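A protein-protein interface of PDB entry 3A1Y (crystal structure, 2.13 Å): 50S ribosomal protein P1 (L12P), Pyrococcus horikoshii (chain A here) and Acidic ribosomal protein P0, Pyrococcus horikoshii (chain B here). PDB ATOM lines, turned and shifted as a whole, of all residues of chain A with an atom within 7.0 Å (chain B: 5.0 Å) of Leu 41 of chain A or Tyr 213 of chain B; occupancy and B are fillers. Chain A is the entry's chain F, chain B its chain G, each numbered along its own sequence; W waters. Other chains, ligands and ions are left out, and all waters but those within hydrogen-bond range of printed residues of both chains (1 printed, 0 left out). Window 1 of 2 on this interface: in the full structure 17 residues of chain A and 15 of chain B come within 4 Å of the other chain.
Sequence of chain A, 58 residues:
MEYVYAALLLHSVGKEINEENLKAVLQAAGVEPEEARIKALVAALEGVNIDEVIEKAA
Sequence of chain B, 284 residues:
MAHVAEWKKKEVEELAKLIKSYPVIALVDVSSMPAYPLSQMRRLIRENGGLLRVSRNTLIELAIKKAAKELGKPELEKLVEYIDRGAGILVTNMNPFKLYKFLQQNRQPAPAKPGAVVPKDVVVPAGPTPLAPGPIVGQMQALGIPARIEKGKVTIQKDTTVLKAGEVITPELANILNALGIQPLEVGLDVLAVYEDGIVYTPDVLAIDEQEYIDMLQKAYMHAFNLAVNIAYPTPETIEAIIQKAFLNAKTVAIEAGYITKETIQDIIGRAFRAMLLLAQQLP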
ATOM      1  N   TYR A   3      21.702  -3.482   7.890  1.00  0.00           N
ATOM      2  CA  TYR A   3      20.948  -4.217   8.924  1.00  0.00           C
ATOM      3  C   TYR A   3      19.685  -4.832   8.327  1.00  0.00           C
ATOM      4  O   TYR A   3      19.309  -5.975   8.610  1.00  0.00           O
ATOM      5  CB  TYR A   3      20.638  -3.304  10.127  1.00  0.00           C
ATOM      6  CG  TYR A   3      21.907  -2.983  10.900  1.00  0.00           C
ATOM      7  CD1 TYR A   3      22.378  -3.840  11.893  1.00  0.00           C
ATOM      8  CD2 TYR A   3      22.659  -1.839  10.601  1.00  0.00           C
ATOM      9  CE1 TYR A   3      23.570  -3.561  12.583  1.00  0.00           C
ATOM     10  CE2 TYR A   3      23.856  -1.560  11.277  1.00  0.00           C
ATOM     11  CZ  TYR A   3      24.300  -2.428  12.262  1.00  0.00           C
ATOM     12  OH  TYR A   3      25.453  -2.144  12.916  1.00  0.00           O
ATOM     13  N   VAL A   4      19.060  -4.051   7.471  1.00  0.00           N
ATOM     14  CA  VAL A   4      17.836  -4.444   6.830  1.00  0.00           C
ATOM     15  C   VAL A   4      18.137  -5.478   5.742  1.00  0.00           C
ATOM     16  O   VAL A   4      17.446  -6.462   5.644  1.00  0.00           O
ATOM     17  CB  VAL A   4      17.081  -3.189   6.353  1.00  0.00           C
ATOM     18  CG1 VAL A   4      15.865  -3.564   5.605  1.00  0.00           C
ATOM     19  CG2 VAL A   4      16.638  -2.386   7.606  1.00  0.00           C
ATOM     20  N   ALA A   6      20.771  -7.460   5.797  1.00  0.00           N
ATOM     21  CA  ALA A   6      21.151  -8.662   6.559  1.00  0.00           C
ATOM     22  C   ALA A   6      19.894  -9.463   7.000  1.00  0.00           C
ATOM     23  O   ALA A   6      19.890 -10.691   6.920  1.00  0.00           O
ATOM     24  CB  ALA A   6      21.991  -8.277   7.760  1.00  0.00           C
ATOM     25  N   ALA A   7      18.843  -8.754   7.441  1.00  0.00           N
ATOM     26  CA  ALA A   7      17.583  -9.364   7.898  1.00  0.00           C
ATOM     27  C   ALA A   7      16.861 -10.046   6.750  1.00  0.00           C
ATOM     28  O   ALA A   7      16.349 -11.167   6.886  1.00  0.00           O
ATOM     29  CB  ALA A   7      16.661  -8.289   8.501  1.00  0.00           C
ATOM     30  N   ILE A  17      16.124 -14.261  12.342  1.00  0.00           N
ATOM     31  CA  ILE A  17      16.712 -12.968  12.521  1.00  0.00           C
ATOM     32  C   ILE A  17      16.920 -12.754  14.018  1.00  0.00           C
ATOM     33  O   ILE A  17      16.060 -12.210  14.724  1.00  0.00           O
ATOM     34  CB  ILE A  17      15.836 -11.860  11.880  1.00  0.00           C
ATOM     35  CG1 ILE A  17      15.674 -12.132  10.377  1.00  0.00           C
ATOM     36  CG2 ILE A  17      16.461 -10.485  12.104  1.00  0.00           C
ATOM     37  CD1 ILE A  17      14.534 -11.407   9.721  1.00  0.00           C
ATOM     38  N   ASN A  18      18.071 -13.209  14.495  1.00  0.00           N
ATOM     39  CA  ASN A  18      18.452 -13.036  15.887  1.00  0.00           C
ATOM     40  C   ASN A  18      19.819 -12.382  15.936  1.00  0.00           C
ATOM     41  O   ASN A  18      20.444 -12.175  14.901  1.00  0.00           O
ATOM     42  CB  ASN A  18      18.407 -14.381  16.670  1.00  0.00           C
ATOM     43  CG  ASN A  18      19.371 -15.448  16.123  1.00  0.00           C
ATOM     44  OD1 ASN A  18      19.141 -16.646  16.323  1.00  0.00           O
ATOM     45  ND2 ASN A  18      20.445 -15.033  15.465  1.00  0.00           N
ATOM     46  N   LEU A  22      22.542 -12.334  12.731  1.00  0.00           N
ATOM     47  CA  LEU A  22      22.773 -11.007  12.178  1.00  0.00           C
ATOM     48  C   LEU A  22      24.254 -10.612  12.286  1.00  0.00           C
ATOM     49  O   LEU A  22      24.838 -10.129  11.321  1.00  0.00           O
ATOM     50  CB  LEU A  22      21.896  -9.959  12.874  1.00  0.00           C
ATOM     51  CG  LEU A  22      20.460  -9.735  12.421  1.00  0.00           C
ATOM     52  CD1 LEU A  22      19.818  -8.800  13.464  1.00  0.00           C
ATOM     53  CD2 LEU A  22      20.355  -9.093  11.009  1.00  0.00           C
ATOM     54  N   GLU A  35      26.146  -3.174  18.829  1.00  0.00           N
ATOM     55  CA  GLU A  35      25.205  -3.973  19.609  1.00  0.00           C
ATOM     56  C   GLU A  35      23.816  -3.316  19.691  1.00  0.00           C
ATOM     57  O   GLU A  35      22.813  -3.981  19.471  1.00  0.00           O
ATOM     58  CB  GLU A  35      25.793  -4.296  20.993  1.00  0.00           C
ATOM     59  CG  GLU A  35      24.868  -5.048  21.947  1.00  0.00           C
ATOM     60  CD  GLU A  35      24.409  -6.416  21.433  1.00  0.00           C
ATOM     61  OE1 GLU A  35      23.384  -6.914  21.940  1.00  0.00           O
ATOM     62  OE2 GLU A  35      25.052  -7.006  20.534  1.00  0.00           O
ATOM     63  N   ALA A  36      23.779  -2.013  19.962  1.00  0.00           N
ATOM     64  CA  ALA A  36      22.519  -1.274  20.079  1.00  0.00           C
ATOM     65  C   ALA A  36      21.687  -1.353  18.807  1.00  0.00           C
ATOM     66  O   ALA A  36      20.478  -1.453  18.878  1.00  0.00           O
ATOM     67  CB  ALA A  36      22.758   0.198  20.477  1.00  0.00           C
ATOM     68  N   ARG A  37      22.335  -1.297  17.649  1.00  0.00           N
ATOM     69  CA  ARG A  37      21.626  -1.303  16.372  1.00  0.00           C
ATOM     70  C   ARG A  37      21.213  -2.728  16.029  1.00  0.00           C
ATOM     71  O   ARG A  37      20.146  -2.964  15.461  1.00  0.00           O
ATOM     72  CB  ARG A  37      22.515  -0.714  15.267  1.00  0.00           C
ATOM     73  CG  ARG A  37      22.940   0.727  15.542  1.00  0.00           C
ATOM     74  CD  ARG A  37      23.874   1.242  14.452  1.00  0.00           C
ATOM     75  NE  ARG A  37      23.199   1.492  13.177  1.00  0.00           N
ATOM     76  CZ  ARG A  37      23.838   1.881  12.066  1.00  0.00           C
ATOM     77  NH1 ARG A  37      25.171   2.049  12.062  1.00  0.00           N
ATOM     78  NH2 ARG A  37      23.151   2.103  10.962  1.00  0.00           N
ATOM     79  N   ILE A  38      22.056  -3.686  16.393  1.00  0.00           N
ATOM     80  CA  ILE A  38      21.680  -5.088  16.238  1.00  0.00           C
ATOM     81  C   ILE A  38      20.439  -5.410  17.079  1.00  0.00           C
ATOM     82  O   ILE A  38      19.460  -5.975  16.579  1.00  0.00           O
ATOM     83  CB  ILE A  38      22.831  -6.029  16.616  1.00  0.00           C
ATOM     84  CG1 ILE A  38      23.978  -5.906  15.595  1.00  0.00           C
ATOM     85  CG2 ILE A  38      22.340  -7.517  16.605  1.00  0.00           C
ATOM     86  CD1 ILE A  38      25.299  -6.456  16.093  1.00  0.00           C
ATOM     87  N   LYS A  39      20.490  -5.048  18.361  1.00  0.00           N
ATOM     88  CA  LYS A  39      19.411  -5.373  19.284  1.00  0.00           C
ATOM     89  C   LYS A  39      18.140  -4.613  18.900  1.00  0.00           C
ATOM     90  O   LYS A  39      17.052  -5.171  18.963  1.00  0.00           O
ATOM     91  CB  LYS A  39      19.828  -5.065  20.728  1.00  0.00           C
ATOM     92  CG  LYS A  39      18.964  -5.748  21.784  1.00  0.00           C
ATOM     93  CD  LYS A  39      19.393  -5.342  23.217  1.00  0.00           C
ATOM     94  CE  LYS A  39      20.769  -5.889  23.586  1.00  0.00           C
ATOM     95  NZ  LYS A  39      20.914  -7.363  23.435  1.00  0.00           N
ATOM     96  N   ALA A  40      18.287  -3.350  18.491  1.00  0.00           N
ATOM     97  CA  ALA A  40      17.148  -2.545  18.055  1.00  0.00           C
ATOM     98  C   ALA A  40      16.447  -3.204  16.849  1.00  0.00           C
ATOM     99  O   ALA A  40      15.226  -3.254  16.782  1.00  0.00           O
ATOM    100  CB  ALA A  40      17.602  -1.124  17.702  1.00  0.00           C
ATOM    101  N   LEU A  41      17.238  -3.700  15.901  1.00  0.00           N
ATOM    102  CA  LEU A  41      16.706  -4.333  14.686  1.00  0.00           C
ATOM    103  C   LEU A  41      15.901  -5.578  15.072  1.00  0.00           C
ATOM    104  O   LEU A  41      14.764  -5.776  14.626  1.00  0.00           O
ATOM    105  CB  LEU A  41      17.857  -4.678  13.732  1.00  0.00           C
ATOM    106  CG  LEU A  41      17.579  -5.151  12.284  1.00  0.00           C
ATOM    107  CD1 LEU A  41      17.502  -6.665  12.199  1.00  0.00           C
ATOM    108  CD2 LEU A  41      16.309  -4.517  11.678  1.00  0.00           C
ATOM    109  N   VAL A  42      16.491  -6.412  15.921  1.00  0.00           N
ATOM    110  CA  VAL A  42      15.799  -7.600  16.420  1.00  0.00           C
ATOM    111  C   VAL A  42      14.504  -7.237  17.159  1.00  0.00           C
ATOM    112  O   VAL A  42      13.464  -7.862  16.937  1.00  0.00           O
ATOM    113  CB  VAL A  42      16.729  -8.472  17.288  1.00  0.00           C
ATOM    114  CG1 VAL A  42      15.965  -9.622  17.919  1.00  0.00           C
ATOM    115  CG2 VAL A  42      17.865  -9.017  16.433  1.00  0.00           C
ATOM    116  N   ALA A  43      14.542  -6.223  18.015  1.00  0.00           N
ATOM    117  CA  ALA A  43      13.323  -5.803  18.721  1.00  0.00           C
ATOM    118  C   ALA A  43      12.265  -5.297  17.737  1.00  0.00           C
ATOM    119  O   ALA A  43      11.102  -5.642  17.849  1.00  0.00           O
ATOM    120  CB  ALA A  43      13.635  -4.746  19.775  1.00  0.00           C
ATOM    121  N   ALA A  44      12.682  -4.485  16.770  1.00  0.00           N
ATOM    122  CA  ALA A  44      11.758  -3.926  15.791  1.00  0.00           C
ATOM    123  C   ALA A  44      11.053  -5.014  14.972  1.00  0.00           C
ATOM    124  O   ALA A  44       9.888  -4.863  14.599  1.00  0.00           O
ATOM    125  CB  ALA A  44      12.494  -2.945  14.854  1.00  0.00           C
ATOM    126  N   LEU A  45      11.768  -6.101  14.695  1.00  0.00           N
ATOM    127  CA  LEU A  45      11.266  -7.164  13.825  1.00  0.00           C
ATOM    128  C   LEU A  45      10.549  -8.283  14.577  1.00  0.00           C
ATOM    129  O   LEU A  45       9.944  -9.155  13.955  1.00  0.00           O
ATOM    130  CB  LEU A  45      12.399  -7.710  12.935  1.00  0.00           C
ATOM    131  CG  LEU A  45      12.530  -7.212  11.487  1.00  0.00           C
ATOM    132  CD1 LEU A  45      11.909  -5.836  11.179  1.00  0.00           C
ATOM    133  CD2 LEU A  45      13.980  -7.244  11.014  1.00  0.00           C
ATOM    134  N   GLU A  46      10.590  -8.240  15.908  1.00  0.00           N
ATOM    135  CA  GLU A  46       9.854  -9.195  16.746  1.00  0.00           C
ATOM    136  C   GLU A  46       8.346  -9.073  16.533  1.00  0.00           C
ATOM    137  O   GLU A  46       7.779  -7.981  16.624  1.00  0.00           O
ATOM    138  CB  GLU A  46      10.176  -8.985  18.227  1.00  0.00           C
ATOM    139  CG  GLU A  46      10.520 -10.275  18.973  1.00  0.00           C
ATOM    140  CD  GLU A  46      12.017 -10.621  18.882  1.00  0.00           C
ATOM    141  OE1 GLU A  46      12.558 -10.730  17.740  1.00  0.00           O
ATOM    142  OE2 GLU A  46      12.646 -10.777  19.961  1.00  0.00           O
ATOM    143  N   VAL A  53       4.633  -7.943   5.246  1.00  0.00           N
ATOM    144  CA  VAL A  53       5.298  -6.673   4.989  1.00  0.00           C
ATOM    145  C   VAL A  53       5.780  -6.573   3.530  1.00  0.00           C
ATOM    146  O   VAL A  53       5.553  -5.555   2.866  1.00  0.00           O
ATOM    147  CB  VAL A  53       6.475  -6.462   5.985  1.00  0.00           C
ATOM    148  CG1 VAL A  53       7.376  -5.315   5.552  1.00  0.00           C
ATOM    149  CG2 VAL A  53       5.934  -6.204   7.377  1.00  0.00           C
ATOM    150  N   ILE B 208      11.986   2.917  19.787  1.00  0.00           N
ATOM    151  CA  ILE B 208      11.985   2.421  18.403  1.00  0.00           C
ATOM    152  C   ILE B 208      10.854   3.038  17.577  1.00  0.00           C
ATOM    153  O   ILE B 208       9.708   3.077  18.024  1.00  0.00           O
ATOM    154  CB  ILE B 208      11.902   0.845  18.383  1.00  0.00           C
ATOM    155  CG1 ILE B 208      13.284   0.194  18.350  1.00  0.00           C
ATOM    156  CG2 ILE B 208      11.132   0.313  17.171  1.00  0.00           C
ATOM    157  CD1 ILE B 208      14.451   1.111  18.661  1.00  0.00           C
ATOM    158  N   ASP B 209      11.183   3.514  16.377  1.00  0.00           N
ATOM    159  CA  ASP B 209      10.159   3.950  15.419  1.00  0.00           C
ATOM    160  C   ASP B 209       9.796   2.770  14.528  1.00  0.00           C
ATOM    161  O   ASP B 209      10.412   2.542  13.486  1.00  0.00           O
ATOM    162  CB  ASP B 209      10.635   5.147  14.584  1.00  0.00           C
ATOM    163  CG  ASP B 209       9.528   5.743  13.693  1.00  0.00           C
ATOM    164  OD1 ASP B 209       8.495   5.082  13.394  1.00  0.00           O
ATOM    165  OD2 ASP B 209       9.706   6.907  13.281  1.00  0.00           O
ATOM    166  N   GLU B 210       8.781   2.030  14.949  1.00  0.00           N
ATOM    167  CA  GLU B 210       8.409   0.777  14.309  1.00  0.00           C
ATOM    168  C   GLU B 210       8.062   0.947  12.822  1.00  0.00           C
ATOM    169  O   GLU B 210       8.436   0.104  11.987  1.00  0.00           O
ATOM    170  CB  GLU B 210       7.255   0.133  15.094  1.00  0.00           C
ATOM    171  CG  GLU B 210       6.884  -1.290  14.697  1.00  0.00           C
ATOM    172  CD  GLU B 210       8.021  -2.302  14.866  1.00  0.00           C
ATOM    173  OE1 GLU B 210       8.892  -2.127  15.736  1.00  0.00           O
ATOM    174  OE2 GLU B 210       8.031  -3.297  14.124  1.00  0.00           O
ATOM    175  N   GLN B 211       7.362   2.029  12.484  1.00  0.00           N
ATOM    176  CA  GLN B 211       6.993   2.267  11.086  1.00  0.00           C
ATOM    177  C   GLN B 211       8.215   2.569  10.201  1.00  0.00           C
ATOM    178  O   GLN B 211       8.245   2.186   9.037  1.00  0.00           O
ATOM    179  CB  GLN B 211       5.900   3.351  10.965  1.00  0.00           C
ATOM    180  CG  GLN B 211       5.199   3.422   9.589  1.00  0.00           C
ATOM    181  CD  GLN B 211       4.588   2.089   9.139  1.00  0.00           C
ATOM    182  OE1 GLN B 211       4.909   1.581   8.062  1.00  0.00           O
ATOM    183  NE2 GLN B 211       3.717   1.519   9.965  1.00  0.00           N
ATOM    184  N   GLU B 212       9.213   3.250  10.762  1.00  0.00           N
ATOM    185  CA  GLU B 212      10.483   3.508  10.080  1.00  0.00           C
ATOM    186  C   GLU B 212      11.178   2.203   9.705  1.00  0.00           C
ATOM    187  O   GLU B 212      11.676   2.056   8.596  1.00  0.00           O
ATOM    188  CB  GLU B 212      11.395   4.343  10.978  1.00  0.00           C
ATOM    189  CG  GLU B 212      12.725   4.808  10.376  1.00  0.00           C
ATOM    190  CD  GLU B 212      13.584   5.517  11.434  1.00  0.00           C
ATOM    191  OE1 GLU B 212      14.330   4.821  12.182  1.00  0.00           O
ATOM    192  OE2 GLU B 212      13.476   6.766  11.545  1.00  0.00           O
ATOM    193  N   TYR B 213      11.222   1.260  10.638  1.00  0.00           N
ATOM    194  CA  TYR B 213      11.804  -0.054  10.349  1.00  0.00           C
ATOM    195  C   TYR B 213      11.011  -0.803   9.282  1.00  0.00           C
ATOM    196  O   TYR B 213      11.592  -1.439   8.426  1.00  0.00           O
ATOM    197  CB  TYR B 213      11.898  -0.892  11.611  1.00  0.00           C
ATOM    198  CG  TYR B 213      13.128  -0.608  12.432  1.00  0.00           C
ATOM    199  CD1 TYR B 213      13.118   0.377  13.433  1.00  0.00           C
ATOM    200  CD2 TYR B 213      14.302  -1.336  12.223  1.00  0.00           C
ATOM    201  CE1 TYR B 213      14.251   0.628  14.207  1.00  0.00           C
ATOM    202  CE2 TYR B 213      15.436  -1.104  12.989  1.00  0.00           C
ATOM    203  CZ  TYR B 213      15.409  -0.122  13.973  1.00  0.00           C
ATOM    204  OH  TYR B 213      16.541   0.094  14.714  1.00  0.00           O
ATOM    205  N   ILE B 214       9.685  -0.708   9.337  1.00  0.00           N
ATOM    206  CA  ILE B 214       8.820  -1.368   8.357  1.00  0.00           C
ATOM    207  C   ILE B 214       9.024  -0.756   6.983  1.00  0.00           C
ATOM    208  O   ILE B 214       9.164  -1.481   6.002  1.00  0.00           O
ATOM    209  CB  ILE B 214       7.328  -1.305   8.749  1.00  0.00           C
ATOM    210  CG1 ILE B 214       7.074  -2.003  10.108  1.00  0.00           C
ATOM    211  CG2 ILE B 214       6.413  -1.850   7.617  1.00  0.00           C
ATOM    212  CD1 ILE B 214       7.627  -3.423  10.220  1.00  0.00           C
ATOM    213  N   ASP B 215       9.040   0.580   6.935  1.00  0.00           N
ATOM    214  CA  ASP B 215       9.309   1.309   5.699  1.00  0.00           C
ATOM    215  C   ASP B 215      10.672   0.951   5.101  1.00  0.00           C
ATOM    216  O   ASP B 215      10.801   0.842   3.891  1.00  0.00           O
ATOM    217  CB  ASP B 215       9.241   2.823   5.910  1.00  0.00           C
ATOM    218  CG  ASP B 215       7.853   3.302   6.307  1.00  0.00           C
ATOM    219  OD1 ASP B 215       6.853   2.599   6.033  1.00  0.00           O
ATOM    220  OD2 ASP B 215       7.771   4.392   6.910  1.00  0.00           O
ATOM    221  N   MET B 216      11.681   0.786   5.946  1.00  0.00           N
ATOM    222  CA  MET B 216      13.031   0.534   5.452  1.00  0.00           C
ATOM    223  C   MET B 216      13.132  -0.878   4.908  1.00  0.00           C
ATOM    224  O   MET B 216      13.807  -1.141   3.899  1.00  0.00           O
ATOM    225  CB  MET B 216      14.057   0.740   6.564  1.00  0.00           C
ATOM    226  CG  MET B 216      14.260   2.224   6.941  1.00  0.00           C
ATOM    227  SD  MET B 216      15.446   2.447   8.299  1.00  0.00           S
ATOM    228  CE  MET B 216      16.864   1.665   7.631  1.00  0.00           C
ATOM    229  N   LEU B 217      12.460  -1.794   5.595  1.00  0.00           N
ATOM    230  CA  LEU B 217      12.381  -3.179   5.140  1.00  0.00           C
ATOM    231  C   LEU B 217      11.757  -3.282   3.758  1.00  0.00           C
ATOM    232  O   LEU B 217      12.273  -3.982   2.898  1.00  0.00           O
ATOM    233  CB  LEU B 217      11.594  -4.012   6.145  1.00  0.00           C
ATOM    234  CG  LEU B 217      11.845  -5.509   6.192  1.00  0.00           C
ATOM    235  CD1 LEU B 217      13.233  -5.832   6.674  1.00  0.00           C
ATOM    236  CD2 LEU B 217      10.789  -6.107   7.139  1.00  0.00           C
HETATM  237  O   HOH W   1      18.641  -1.096  14.073  1.00  0.00           O
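Tyr 3 of chain A touches none of the printed residues of chain B.
Printed residues of chain B within 4 Å of Val 4 of chain A: Met 216 (3.6 Å) and Leu 217 (3.5 Å).
Of the printed residues of chain B, Ala 40 of chain A touches Ile 208 (3.98 Å) and Tyr 213 (3.4 Å).
Of chain B, only Tyr 213 comes within 4 Å of Leu 41 of chain A.
Printed residues of chain A within 4 Å of Ile 208 of chain B: Ala 40 (3.98 Å).
Of the printed residues of chain A, Tyr 213 of chain B touches Ala 40 (3.4 Å), Leu 41 (3.8 Å) and Ala 44 (3.4 Å).
Of the printed residues of chain A, Leu 217 of chain B touches Val 4 and Val 53.
The nearest printed residue of chain B that does not touch Leu 41 of chain A is Leu 217 of chain B (6.0 Å).
The nearest printed residue of chain B that does not touch Val 4 of chain A is Tyr 213 of chain B (5.2 Å).
Of the 20 printed residues of chain A, 5 touch a printed residue of chain B.
Printed residues of chain A that touch a printed residue of chain B: Val 4, Ala 40, Leu 41, Ala 44 and Val 53.
Hydrophobic or aromatic side chains of chain B that line the printed part of chain A: Ile 208, Tyr 213 and Leu 217.
Among the printed residues, 8 pairs touch across the chains.
Among the printed residues, no Asp or Glu carboxylate lies within 4 Å of a Lys or Arg side-chain nitrogen of the other chain.
The side-chain carboxylate (OE2) of Glu 210 of chain B lies close to the backbone carbonyl oxygen (O) of Ala 44 of chain A (2.5 Å).
Water W1 lies within hydrogen-bond range of the side-chain hydroxyl (OH) of Tyr 213 of chain B (2.5 Å), the backbone carbonyl oxygen (O) of Arg 37 of chain A (2.8 Å) and the backbone NH (N) of Leu 41 of chain A (3.5 Å).
O of Met 216 of chain B touches CG1 of Val 4 of chain A, at 3.6 Å.
Val 4 of chain A touches Leu 217 of chain B.
CD1 of Ile 208 of chain B touches CB of Ala 40 of chain A, 3.98 Å away.
OH of Tyr 213 of chain B touches CB of Ala 40 of chain A, 3.4 Å away.
CD2 of Leu 41 of chain A touches CE2 of Tyr 213 of chain B, 3.8 Å away.
CG of Tyr 213 of chain B touches CB of Ala 44 of chain A, at 3.4 Å.
Leu 217 of chain B touches Val 53 of chain A (CD2 to CG1, 3.8 Å).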
